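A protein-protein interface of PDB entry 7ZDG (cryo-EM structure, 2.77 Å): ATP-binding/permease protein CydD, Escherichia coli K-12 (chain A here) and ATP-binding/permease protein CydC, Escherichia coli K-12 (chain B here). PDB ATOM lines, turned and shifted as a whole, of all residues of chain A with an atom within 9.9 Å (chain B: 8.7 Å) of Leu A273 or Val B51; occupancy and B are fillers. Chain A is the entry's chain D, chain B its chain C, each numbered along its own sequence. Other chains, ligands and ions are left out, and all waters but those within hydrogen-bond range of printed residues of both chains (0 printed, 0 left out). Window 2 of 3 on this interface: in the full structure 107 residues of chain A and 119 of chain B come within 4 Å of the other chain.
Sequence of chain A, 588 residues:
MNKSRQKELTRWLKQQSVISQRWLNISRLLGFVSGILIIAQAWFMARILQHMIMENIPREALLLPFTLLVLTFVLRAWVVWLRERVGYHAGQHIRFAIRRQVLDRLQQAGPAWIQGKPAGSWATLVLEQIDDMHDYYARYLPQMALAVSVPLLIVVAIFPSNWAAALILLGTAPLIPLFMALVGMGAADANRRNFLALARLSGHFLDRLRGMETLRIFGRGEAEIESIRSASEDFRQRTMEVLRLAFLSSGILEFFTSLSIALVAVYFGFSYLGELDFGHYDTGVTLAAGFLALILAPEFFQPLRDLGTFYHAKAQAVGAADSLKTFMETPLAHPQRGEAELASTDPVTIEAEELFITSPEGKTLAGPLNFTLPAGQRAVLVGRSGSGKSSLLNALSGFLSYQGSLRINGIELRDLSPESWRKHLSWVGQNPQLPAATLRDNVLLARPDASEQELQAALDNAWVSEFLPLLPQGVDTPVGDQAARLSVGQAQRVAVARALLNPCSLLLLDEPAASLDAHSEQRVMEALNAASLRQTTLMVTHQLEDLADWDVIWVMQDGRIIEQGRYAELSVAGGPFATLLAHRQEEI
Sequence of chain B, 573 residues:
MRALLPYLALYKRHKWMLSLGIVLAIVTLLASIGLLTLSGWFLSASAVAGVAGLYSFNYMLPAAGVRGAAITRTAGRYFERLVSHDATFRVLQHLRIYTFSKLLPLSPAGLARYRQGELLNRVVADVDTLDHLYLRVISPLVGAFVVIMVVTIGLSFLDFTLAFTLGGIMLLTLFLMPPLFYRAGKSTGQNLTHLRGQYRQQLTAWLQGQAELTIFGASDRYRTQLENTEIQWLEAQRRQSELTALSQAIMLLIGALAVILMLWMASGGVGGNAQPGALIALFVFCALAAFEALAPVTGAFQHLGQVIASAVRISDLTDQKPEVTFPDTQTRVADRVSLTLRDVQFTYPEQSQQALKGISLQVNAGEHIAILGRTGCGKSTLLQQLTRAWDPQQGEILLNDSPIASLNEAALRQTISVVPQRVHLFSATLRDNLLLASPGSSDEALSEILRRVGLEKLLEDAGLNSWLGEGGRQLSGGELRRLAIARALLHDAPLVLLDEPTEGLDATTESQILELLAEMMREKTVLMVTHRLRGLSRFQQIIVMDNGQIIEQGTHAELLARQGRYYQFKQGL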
ATOM      1  N   MET A  54      20.982 -37.146 -12.381  1.00  0.00           N
ATOM      2  CA  MET A  54      20.688 -38.078 -11.300  1.00  0.00           C
ATOM      3  C   MET A  54      20.902 -39.531 -11.712  1.00  0.00           C
ATOM      4  O   MET A  54      21.673 -40.251 -11.074  1.00  0.00           O
ATOM      5  CB  MET A  54      19.252 -37.878 -10.810  1.00  0.00           C
ATOM      6  CG  MET A  54      19.008 -36.535 -10.160  1.00  0.00           C
ATOM      7  SD  MET A  54      20.014 -36.252  -8.698  1.00  0.00           S
ATOM      8  CE  MET A  54      19.290 -37.427  -7.567  1.00  0.00           C
ATOM      9  N   ALA A 265      14.352 -21.780  -5.973  1.00  0.00           N
ATOM     10  CA  ALA A 265      15.640 -22.438  -5.795  1.00  0.00           C
ATOM     11  C   ALA A 265      15.853 -22.854  -4.347  1.00  0.00           C
ATOM     12  O   ALA A 265      16.336 -23.957  -4.071  1.00  0.00           O
ATOM     13  CB  ALA A 265      16.766 -21.517  -6.254  1.00  0.00           C
ATOM     14  N   VAL A 266      15.509 -21.975  -3.407  1.00  0.00           N
ATOM     15  CA  VAL A 266      15.742 -22.263  -1.997  1.00  0.00           C
ATOM     16  C   VAL A 266      14.810 -23.365  -1.513  1.00  0.00           C
ATOM     17  O   VAL A 266      15.233 -24.291  -0.814  1.00  0.00           O
ATOM     18  CB  VAL A 266      15.589 -20.980  -1.162  1.00  0.00           C
ATOM     19  CG1 VAL A 266      15.309 -21.316   0.284  1.00  0.00           C
ATOM     20  CG2 VAL A 266      16.835 -20.140  -1.275  1.00  0.00           C
ATOM     21  N   TYR A 267      13.532 -23.289  -1.881  1.00  0.00           N
ATOM     22  CA  TYR A 267      12.580 -24.298  -1.432  1.00  0.00           C
ATOM     23  C   TYR A 267      12.963 -25.678  -1.942  1.00  0.00           C
ATOM     24  O   TYR A 267      13.040 -26.639  -1.171  1.00  0.00           O
ATOM     25  CB  TYR A 267      11.170 -23.942  -1.892  1.00  0.00           C
ATOM     26  CG  TYR A 267      10.265 -25.141  -1.968  1.00  0.00           C
ATOM     27  CD1 TYR A 267       9.777 -25.736  -0.818  1.00  0.00           C
ATOM     28  CD2 TYR A 267       9.907 -25.686  -3.184  1.00  0.00           C
ATOM     29  CE1 TYR A 267       8.958 -26.835  -0.881  1.00  0.00           C
ATOM     30  CE2 TYR A 267       9.091 -26.785  -3.255  1.00  0.00           C
ATOM     31  CZ  TYR A 267       8.620 -27.356  -2.102  1.00  0.00           C
ATOM     32  OH  TYR A 267       7.803 -28.454  -2.174  1.00  0.00           O
ATOM     33  N   PHE A 268      13.198 -25.798  -3.246  1.00  0.00           N
ATOM     34  CA  PHE A 268      13.547 -27.094  -3.812  1.00  0.00           C
ATOM     35  C   PHE A 268      14.908 -27.561  -3.322  1.00  0.00           C
ATOM     36  O   PHE A 268      15.093 -28.742  -3.015  1.00  0.00           O
ATOM     37  CB  PHE A 268      13.523 -27.022  -5.336  1.00  0.00           C
ATOM     38  CG  PHE A 268      12.164 -27.209  -5.925  1.00  0.00           C
ATOM     39  CD1 PHE A 268      11.472 -26.138  -6.449  1.00  0.00           C
ATOM     40  CD2 PHE A 268      11.579 -28.455  -5.955  1.00  0.00           C
ATOM     41  CE1 PHE A 268      10.227 -26.310  -6.990  1.00  0.00           C
ATOM     42  CE2 PHE A 268      10.334 -28.629  -6.495  1.00  0.00           C
ATOM     43  CZ  PHE A 268       9.658 -27.556  -7.014  1.00  0.00           C
ATOM     44  N   GLY A 269      15.872 -26.646  -3.234  1.00  0.00           N
ATOM     45  CA  GLY A 269      17.214 -27.039  -2.840  1.00  0.00           C
ATOM     46  C   GLY A 269      17.270 -27.611  -1.438  1.00  0.00           C
ATOM     47  O   GLY A 269      17.972 -28.588  -1.181  1.00  0.00           O
ATOM     48  N   PHE A 270      16.535 -27.002  -0.510  1.00  0.00           N
ATOM     49  CA  PHE A 270      16.528 -27.508   0.856  1.00  0.00           C
ATOM     50  C   PHE A 270      15.592 -28.697   1.013  1.00  0.00           C
ATOM     51  O   PHE A 270      15.753 -29.488   1.946  1.00  0.00           O
ATOM     52  CB  PHE A 270      16.161 -26.389   1.823  1.00  0.00           C
ATOM     53  CG  PHE A 270      17.281 -25.430   2.063  1.00  0.00           C
ATOM     54  CD1 PHE A 270      18.376 -25.806   2.813  1.00  0.00           C
ATOM     55  CD2 PHE A 270      17.254 -24.162   1.520  1.00  0.00           C
ATOM     56  CE1 PHE A 270      19.414 -24.934   3.026  1.00  0.00           C
ATOM     57  CE2 PHE A 270      18.292 -23.287   1.730  1.00  0.00           C
ATOM     58  CZ  PHE A 270      19.371 -23.673   2.484  1.00  0.00           C
ATOM     59  N   SER A 271      14.613 -28.841   0.123  1.00  0.00           N
ATOM     60  CA  SER A 271      13.813 -30.058   0.112  1.00  0.00           C
ATOM     61  C   SER A 271      14.665 -31.263  -0.251  1.00  0.00           C
ATOM     62  O   SER A 271      14.507 -32.341   0.330  1.00  0.00           O
ATOM     63  CB  SER A 271      12.649 -29.911  -0.863  1.00  0.00           C
ATOM     64  OG  SER A 271      11.893 -28.754  -0.569  1.00  0.00           O
ATOM     65  N   TYR A 272      15.570 -31.102  -1.219  1.00  0.00           N
ATOM     66  CA  TYR A 272      16.485 -32.183  -1.568  1.00  0.00           C
ATOM     67  C   TYR A 272      17.415 -32.508  -0.410  1.00  0.00           C
ATOM     68  O   TYR A 272      17.692 -33.681  -0.137  1.00  0.00           O
ATOM     69  CB  TYR A 272      17.291 -31.811  -2.809  1.00  0.00           C
ATOM     70  CG  TYR A 272      16.444 -31.557  -4.028  1.00  0.00           C
ATOM     71  CD1 TYR A 272      15.396 -32.397  -4.347  1.00  0.00           C
ATOM     72  CD2 TYR A 272      16.698 -30.483  -4.862  1.00  0.00           C
ATOM     73  CE1 TYR A 272      14.622 -32.169  -5.450  1.00  0.00           C
ATOM     74  CE2 TYR A 272      15.924 -30.248  -5.968  1.00  0.00           C
ATOM     75  CZ  TYR A 272      14.890 -31.096  -6.257  1.00  0.00           C
ATOM     76  OH  TYR A 272      14.112 -30.873  -7.362  1.00  0.00           O
ATOM     77  N   LEU A 273      17.907 -31.482   0.281  1.00  0.00           N
ATOM     78  CA  LEU A 273      18.791 -31.683   1.419  1.00  0.00           C
ATOM     79  C   LEU A 273      18.080 -32.291   2.618  1.00  0.00           C
ATOM     80  O   LEU A 273      18.752 -32.779   3.531  1.00  0.00           O
ATOM     81  CB  LEU A 273      19.432 -30.354   1.813  1.00  0.00           C
ATOM     82  CG  LEU A 273      20.497 -29.830   0.853  1.00  0.00           C
ATOM     83  CD1 LEU A 273      21.197 -28.625   1.438  1.00  0.00           C
ATOM     84  CD2 LEU A 273      21.496 -30.913   0.523  1.00  0.00           C
ATOM     85  N   GLY A 274      16.750 -32.286   2.636  1.00  0.00           N
ATOM     86  CA  GLY A 274      15.990 -32.836   3.736  1.00  0.00           C
ATOM     87  C   GLY A 274      15.503 -31.829   4.752  1.00  0.00           C
ATOM     88  O   GLY A 274      14.808 -32.218   5.697  1.00  0.00           O
ATOM     89  N   GLU A 275      15.840 -30.548   4.589  1.00  0.00           N
ATOM     90  CA  GLU A 275      15.425 -29.543   5.562  1.00  0.00           C
ATOM     91  C   GLU A 275      13.913 -29.362   5.578  1.00  0.00           C
ATOM     92  O   GLU A 275      13.311 -29.224   6.647  1.00  0.00           O
ATOM     93  CB  GLU A 275      16.119 -28.216   5.269  1.00  0.00           C
ATOM     94  CG  GLU A 275      17.572 -28.186   5.689  1.00  0.00           C
ATOM     95  CD  GLU A 275      17.732 -28.126   7.193  1.00  0.00           C
ATOM     96  OE1 GLU A 275      16.862 -27.529   7.860  1.00  0.00           O
ATOM     97  OE2 GLU A 275      18.725 -28.679   7.710  1.00  0.00           O
ATOM     98  N   LEU A 276      13.282 -29.356   4.409  1.00  0.00           N
ATOM     99  CA  LEU A 276      11.852 -29.121   4.294  1.00  0.00           C
ATOM    100  C   LEU A 276      11.141 -30.401   3.875  1.00  0.00           C
ATOM    101  O   LEU A 276      11.717 -31.258   3.202  1.00  0.00           O
ATOM    102  CB  LEU A 276      11.556 -28.011   3.283  1.00  0.00           C
ATOM    103  CG  LEU A 276      12.305 -26.698   3.499  1.00  0.00           C
ATOM    104  CD1 LEU A 276      12.091 -25.765   2.332  1.00  0.00           C
ATOM    105  CD2 LEU A 276      11.876 -26.047   4.791  1.00  0.00           C
ATOM    106  N   ASP A 277       9.880 -30.531   4.294  1.00  0.00           N
ATOM    107  CA  ASP A 277       9.107 -31.724   3.976  1.00  0.00           C
ATOM    108  C   ASP A 277       7.661 -31.380   3.631  1.00  0.00           C
ATOM    109  O   ASP A 277       6.745 -32.143   3.957  1.00  0.00           O
ATOM    110  CB  ASP A 277       9.148 -32.727   5.130  1.00  0.00           C
ATOM    111  CG  ASP A 277       8.819 -34.141   4.689  1.00  0.00           C
ATOM    112  OD1 ASP A 277       9.025 -35.073   5.493  1.00  0.00           O
ATOM    113  OD2 ASP A 277       8.366 -34.326   3.541  1.00  0.00           O
ATOM    114  N   VAL A 285       9.959 -35.210  -3.658  1.00  0.00           N
ATOM    115  CA  VAL A 285      10.340 -34.144  -4.574  1.00  0.00           C
ATOM    116  C   VAL A 285      11.492 -34.630  -5.439  1.00  0.00           C
ATOM    117  O   VAL A 285      12.478 -35.183  -4.943  1.00  0.00           O
ATOM    118  CB  VAL A 285      10.698 -32.861  -3.801  1.00  0.00           C
ATOM    119  CG1 VAL A 285      11.813 -33.116  -2.809  1.00  0.00           C
ATOM    120  CG2 VAL A 285      11.079 -31.752  -4.758  1.00  0.00           C
ATOM    121  N   LEU A 287      14.203 -34.041  -8.962  1.00  0.00           N
ATOM    122  CA  LEU A 287      14.948 -32.995  -9.649  1.00  0.00           C
ATOM    123  C   LEU A 287      14.192 -32.509 -10.878  1.00  0.00           C
ATOM    124  O   LEU A 287      14.305 -31.342 -11.266  1.00  0.00           O
ATOM    125  CB  LEU A 287      16.337 -33.500 -10.026  1.00  0.00           C
ATOM    126  CG  LEU A 287      17.321 -32.442 -10.512  1.00  0.00           C
ATOM    127  CD1 LEU A 287      17.358 -31.275  -9.553  1.00  0.00           C
ATOM    128  CD2 LEU A 287      18.701 -33.025 -10.692  1.00  0.00           C
ATOM    129  N   PHE B  42      22.452 -24.695  -7.950  1.00  0.00           N
ATOM    130  CA  PHE B  42      22.121 -25.017  -6.566  1.00  0.00           C
ATOM    131  C   PHE B  42      21.138 -26.175  -6.478  1.00  0.00           C
ATOM    132  O   PHE B  42      21.256 -27.028  -5.592  1.00  0.00           O
ATOM    133  CB  PHE B  42      21.559 -23.790  -5.858  1.00  0.00           C
ATOM    134  CG  PHE B  42      21.296 -24.007  -4.403  1.00  0.00           C
ATOM    135  CD1 PHE B  42      22.338 -24.105  -3.507  1.00  0.00           C
ATOM    136  CD2 PHE B  42      20.005 -24.128  -3.932  1.00  0.00           C
ATOM    137  CE1 PHE B  42      22.095 -24.308  -2.173  1.00  0.00           C
ATOM    138  CE2 PHE B  42      19.761 -24.335  -2.599  1.00  0.00           C
ATOM    139  CZ  PHE B  42      20.806 -24.425  -1.719  1.00  0.00           C
ATOM    140  N   LEU B  43      20.145 -26.214  -7.366  1.00  0.00           N
ATOM    141  CA  LEU B  43      19.213 -27.336  -7.377  1.00  0.00           C
ATOM    142  C   LEU B  43      19.929 -28.643  -7.668  1.00  0.00           C
ATOM    143  O   LEU B  43      19.677 -29.659  -7.015  1.00  0.00           O
ATOM    144  CB  LEU B  43      18.108 -27.106  -8.405  1.00  0.00           C
ATOM    145  CG  LEU B  43      16.826 -26.449  -7.917  1.00  0.00           C
ATOM    146  CD1 LEU B  43      17.074 -25.007  -7.650  1.00  0.00           C
ATOM    147  CD2 LEU B  43      15.752 -26.606  -8.952  1.00  0.00           C
ATOM    148  N   SER B  44      20.823 -28.640  -8.654  1.00  0.00           N
ATOM    149  CA  SER B  44      21.518 -29.865  -9.019  1.00  0.00           C
ATOM    150  C   SER B  44      22.489 -30.301  -7.934  1.00  0.00           C
ATOM    151  O   SER B  44      22.549 -31.483  -7.585  1.00  0.00           O
ATOM    152  CB  SER B  44      22.255 -29.669 -10.334  1.00  0.00           C
ATOM    153  OG  SER B  44      21.350 -29.413 -11.377  1.00  0.00           O
ATOM    154  N   ALA B  45      23.270 -29.361  -7.400  1.00  0.00           N
ATOM    155  CA  ALA B  45      24.262 -29.707  -6.390  1.00  0.00           C
ATOM    156  C   ALA B  45      23.604 -30.256  -5.135  1.00  0.00           C
ATOM    157  O   ALA B  45      24.078 -31.239  -4.556  1.00  0.00           O
ATOM    158  CB  ALA B  45      25.112 -28.487  -6.056  1.00  0.00           C
ATOM    159  N   SER B  46      22.513 -29.633  -4.698  1.00  0.00           N
ATOM    160  CA  SER B  46      21.824 -30.108  -3.505  1.00  0.00           C
ATOM    161  C   SER B  46      21.108 -31.425  -3.762  1.00  0.00           C
ATOM    162  O   SER B  46      21.056 -32.289  -2.881  1.00  0.00           O
ATOM    163  CB  SER B  46      20.848 -29.044  -3.016  1.00  0.00           C
ATOM    164  OG  SER B  46      19.817 -28.848  -3.956  1.00  0.00           O
ATOM    165  N   ALA B  47      20.538 -31.595  -4.956  1.00  0.00           N
ATOM    166  CA  ALA B  47      19.889 -32.858  -5.288  1.00  0.00           C
ATOM    167  C   ALA B  47      20.895 -33.997  -5.343  1.00  0.00           C
ATOM    168  O   ALA B  47      20.619 -35.102  -4.865  1.00  0.00           O
ATOM    169  CB  ALA B  47      19.149 -32.739  -6.618  1.00  0.00           C
ATOM    170  N   VAL B  48      22.061 -33.751  -5.938  1.00  0.00           N
ATOM    171  CA  VAL B  48      23.104 -34.770  -5.988  1.00  0.00           C
ATOM    172  C   VAL B  48      23.617 -35.073  -4.587  1.00  0.00           C
ATOM    173  O   VAL B  48      23.825 -36.236  -4.223  1.00  0.00           O
ATOM    174  CB  VAL B  48      24.238 -34.320  -6.924  1.00  0.00           C
ATOM    175  CG1 VAL B  48      25.449 -35.204  -6.750  1.00  0.00           C
ATOM    176  CG2 VAL B  48      23.763 -34.339  -8.359  1.00  0.00           C
ATOM    177  N   ALA B  49      23.830 -34.033  -3.780  1.00  0.00           N
ATOM    178  CA  ALA B  49      24.275 -34.241  -2.407  1.00  0.00           C
ATOM    179  C   ALA B  49      23.239 -35.017  -1.607  1.00  0.00           C
ATOM    180  O   ALA B  49      23.585 -35.923  -0.842  1.00  0.00           O
ATOM    181  CB  ALA B  49      24.570 -32.900  -1.741  1.00  0.00           C
ATOM    182  N   GLY B  50      21.968 -34.680  -1.770  1.00  0.00           N
ATOM    183  CA  GLY B  50      20.920 -35.402  -1.090  1.00  0.00           C
ATOM    184  C   GLY B  50      20.875 -35.082   0.392  1.00  0.00           C
ATOM    185  O   GLY B  50      21.545 -34.184   0.895  1.00  0.00           O
ATOM    186  N   VAL B  51      20.049 -35.858   1.098  1.00  0.00           N
ATOM    187  CA  VAL B  51      19.911 -35.671   2.538  1.00  0.00           C
ATOM    188  C   VAL B  51      21.205 -36.029   3.259  1.00  0.00           C
ATOM    189  O   VAL B  51      21.566 -35.389   4.254  1.00  0.00           O
ATOM    190  CB  VAL B  51      18.714 -36.483   3.063  1.00  0.00           C
ATOM    191  CG1 VAL B  51      18.860 -37.951   2.701  1.00  0.00           C
ATOM    192  CG2 VAL B  51      18.565 -36.307   4.565  1.00  0.00           C
ATOM    193  N   ALA B  52      21.929 -37.040   2.771  1.00  0.00           N
ATOM    194  CA  ALA B  52      23.160 -37.460   3.428  1.00  0.00           C
ATOM    195  C   ALA B  52      24.231 -36.380   3.373  1.00  0.00           C
ATOM    196  O   ALA B  52      25.131 -36.357   4.220  1.00  0.00           O
ATOM    197  CB  ALA B  52      23.677 -38.749   2.793  1.00  0.00           C
ATOM    198  N   GLY B  53      24.159 -35.488   2.393  1.00  0.00           N
ATOM    199  CA  GLY B  53      25.170 -34.464   2.235  1.00  0.00           C
ATOM    200  C   GLY B  53      24.790 -33.119   2.813  1.00  0.00           C
ATOM    201  O   GLY B  53      25.381 -32.100   2.446  1.00  0.00           O
ATOM    202  N   LEU B  54      23.806 -33.094   3.715  1.00  0.00           N
ATOM    203  CA  LEU B  54      23.362 -31.828   4.293  1.00  0.00           C
ATOM    204  C   LEU B  54      24.490 -31.141   5.054  1.00  0.00           C
ATOM    205  O   LEU B  54      24.695 -29.930   4.922  1.00  0.00           O
ATOM    206  CB  LEU B  54      22.162 -32.062   5.213  1.00  0.00           C
ATOM    207  CG  LEU B  54      21.454 -30.824   5.777  1.00  0.00           C
ATOM    208  CD1 LEU B  54      19.968 -31.077   5.902  1.00  0.00           C
ATOM    209  CD2 LEU B  54      22.019 -30.419   7.126  1.00  0.00           C
ATOM    210  N   TYR B  55      25.220 -31.923   5.858  1.00  0.00           N
ATOM    211  CA  TYR B  55      26.308 -31.390   6.724  1.00  0.00           C
ATOM    212  C   TYR B  55      27.528 -30.937   5.910  1.00  0.00           C
ATOM    213  O   TYR B  55      28.188 -29.966   6.330  1.00  0.00           O
ATOM    214  CB  TYR B  55      26.693 -32.401   7.808  1.00  0.00           C
ATOM    215  CG  TYR B  55      27.276 -33.691   7.288  1.00  0.00           C
ATOM    216  CD1 TYR B  55      28.644 -33.843   7.127  1.00  0.00           C
ATOM    217  CD2 TYR B  55      26.464 -34.763   6.956  1.00  0.00           C
ATOM    218  CE1 TYR B  55      29.189 -35.023   6.650  1.00  0.00           C
ATOM    219  CE2 TYR B  55      26.992 -35.950   6.478  1.00  0.00           C
ATOM    220  CZ  TYR B  55      28.360 -36.081   6.324  1.00  0.00           C
ATOM    221  OH  TYR B  55      28.890 -37.248   5.854  1.00  0.00           O
ATOM    222  N   SER B  56      27.855 -31.649   4.828  1.00  0.00           N
ATOM    223  CA  SER B  56      29.004 -31.292   4.002  1.00  0.00           C
ATOM    224  C   SER B  56      28.678 -30.139   3.063  1.00  0.00           C
ATOM    225  O   SER B  56      29.553 -29.329   2.738  1.00  0.00           O
ATOM    226  CB  SER B  56      29.479 -32.508   3.208  1.00  0.00           C
ATOM    227  OG  SER B  56      30.423 -32.128   2.223  1.00  0.00           O
ATOM    228  N   PHE B  57      27.430 -30.052   2.610  1.00  0.00           N
ATOM    229  CA  PHE B  57      27.065 -29.050   1.617  1.00  0.00           C
ATOM    230  C   PHE B  57      27.095 -27.653   2.224  1.00  0.00           C
ATOM    231  O   PHE B  57      26.469 -27.398   3.256  1.00  0.00           O
ATOM    232  CB  PHE B  57      25.679 -29.351   1.048  1.00  0.00           C
ATOM    233  CG  PHE B  57      25.355 -28.574  -0.186  1.00  0.00           C
ATOM    234  CD1 PHE B  57      26.012 -28.834  -1.371  1.00  0.00           C
ATOM    235  CD2 PHE B  57      24.400 -27.580  -0.162  1.00  0.00           C
ATOM    236  CE1 PHE B  57      25.724 -28.115  -2.506  1.00  0.00           C
ATOM    237  CE2 PHE B  57      24.106 -26.861  -1.296  1.00  0.00           C
ATOM    238  CZ  PHE B  57      24.768 -27.128  -2.468  1.00  0.00           C
ATOM    239  N   ASN B  58      27.817 -26.748   1.572  1.00  0.00           N
ATOM    240  CA  ASN B  58      27.890 -25.354   1.980  1.00  0.00           C
ATOM    241  C   ASN B  58      26.878 -24.548   1.181  1.00  0.00           C
ATOM    242  O   ASN B  58      26.927 -24.531  -0.052  1.00  0.00           O
ATOM    243  CB  ASN B  58      29.293 -24.788   1.763  1.00  0.00           C
ATOM    244  CG  ASN B  58      29.442 -23.375   2.293  1.00  0.00           C
ATOM    245  OD1 ASN B  58      28.527 -22.833   2.911  1.00  0.00           O
ATOM    246  ND2 ASN B  58      30.593 -22.768   2.042  1.00  0.00           N
ATOM    247  N   TYR B  59      25.969 -23.877   1.885  1.00  0.00           N
ATOM    248  CA  TYR B  59      24.945 -23.078   1.238  1.00  0.00           C
ATOM    249  C   TYR B  59      24.948 -21.614   1.645  1.00  0.00           C
ATOM    250  O   TYR B  59      24.125 -20.852   1.129  1.00  0.00           O
ATOM    251  CB  TYR B  59      23.552 -23.672   1.501  1.00  0.00           C
ATOM    252  CG  TYR B  59      23.175 -23.773   2.957  1.00  0.00           C
ATOM    253  CD1 TYR B  59      23.305 -24.971   3.640  1.00  0.00           C
ATOM    254  CD2 TYR B  59      22.670 -22.678   3.644  1.00  0.00           C
ATOM    255  CE1 TYR B  59      22.958 -25.074   4.971  1.00  0.00           C
ATOM    256  CE2 TYR B  59      22.320 -22.772   4.975  1.00  0.00           C
ATOM    257  CZ  TYR B  59      22.465 -23.972   5.632  1.00  0.00           C
ATOM    258  OH  TYR B  59      22.117 -24.073   6.959  1.00  0.00           O
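Hydrophobic or aromatic side chains of chain B that line the printed part of chain A: Phe B42, Leu B43, Ala B47, Val B51, Leu B54, Phe B57 and Tyr B59.
Of the 16 printed residues of chain A, 8 touch a printed residue of chain B.
Printed residues of chain A that touch a printed residue of chain B: Met A54, Ala A265, Gly A269, Phe A270, Tyr A272, Leu A273, Glu A275 and Leu A287.
Hydrophobic or aromatic side chains of chain A that line the printed part of chain B: Met A54, Ala A265, Phe A270, Tyr A272, Leu A273 and Leu A287.
Val B51 touches just these residues of chain A: Tyr A272 and Leu A273.
No residue of chain A comes within 4 Å of Ala B49.
Gly B50 touches just these residues of chain A: Tyr A272 (3.5 Å) and Leu A273 (3.3 Å).
No residue of chain A comes within 4 Å of Ala B52.
Of the printed residues of chain B, Met A54 touches Ala B47 (3.8 Å).
Of the printed residues of chain B, Phe A270 touches Tyr B59 (3.6 Å).
Printed residues of chain A within 4 Å of Phe B42: Ala A265 (3.7 Å) and Gly A269 (3.7 Å).
Leu A276 touches none of the printed residues of chain B.
The nearest printed residue of chain A that does not touch Ala B47 is Gly A269 (5.5 Å).
The backbone NH (N) of Val B51 is in hydrogen-bond range of the backbone carbonyl oxygen (O) of Tyr A272.
OG of Ser B46 lies within hydrogen-bond range of O of Gly A269, 3.3 Å away.
Among the printed residues, merely in contact across the chains: Met A54 with Ala B47 (3.8 Å), Ala A265 with Phe B42 (3.7 Å), Ala A265 with Leu B43 (3.5 Å), Gly A269 with Phe B42 (3.7 Å), Phe A270 with Tyr B59 (3.6 Å), Tyr A272 with Leu B43 (3.8 Å), Tyr A272 with Ser B46 (3.6 Å), Tyr A272 with Ala B47 (3.7 Å), Tyr A272 with Gly B50 (3.5 Å), Leu A273 with Ser B46 (3.7 Å), Leu A273 with Gly B50 (3.3 Å), Leu A273 with Val B51 (3.3 Å), Leu A273 with Leu B54 (3.2 Å), Leu A273 with Phe B57 (3.7 Å), Glu A275 with Leu B54 (3.3 Å), Leu A287 with Leu B43 (3.8 Å) and Leu A287 with Ala B47 (3.7 Å).
The backbone NH of Glu A275 lies within hydrogen-bond range of the backbone carbonyl oxygen of Phe A270 (2.8 Å).
The backbone carbonyl oxygen (O) of Phe B42 sits at hydrogen-bond distance from the side-chain hydroxyl (OG) of Ser B46 (2.8 Å).
N of Leu A276 lies within hydrogen-bond range of O of Phe A270.
The backbone carbonyl oxygen (O) of Leu B43 lies within hydrogen-bond range of the side-chain hydroxyl (OG) of Ser B46 (3.2 Å).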
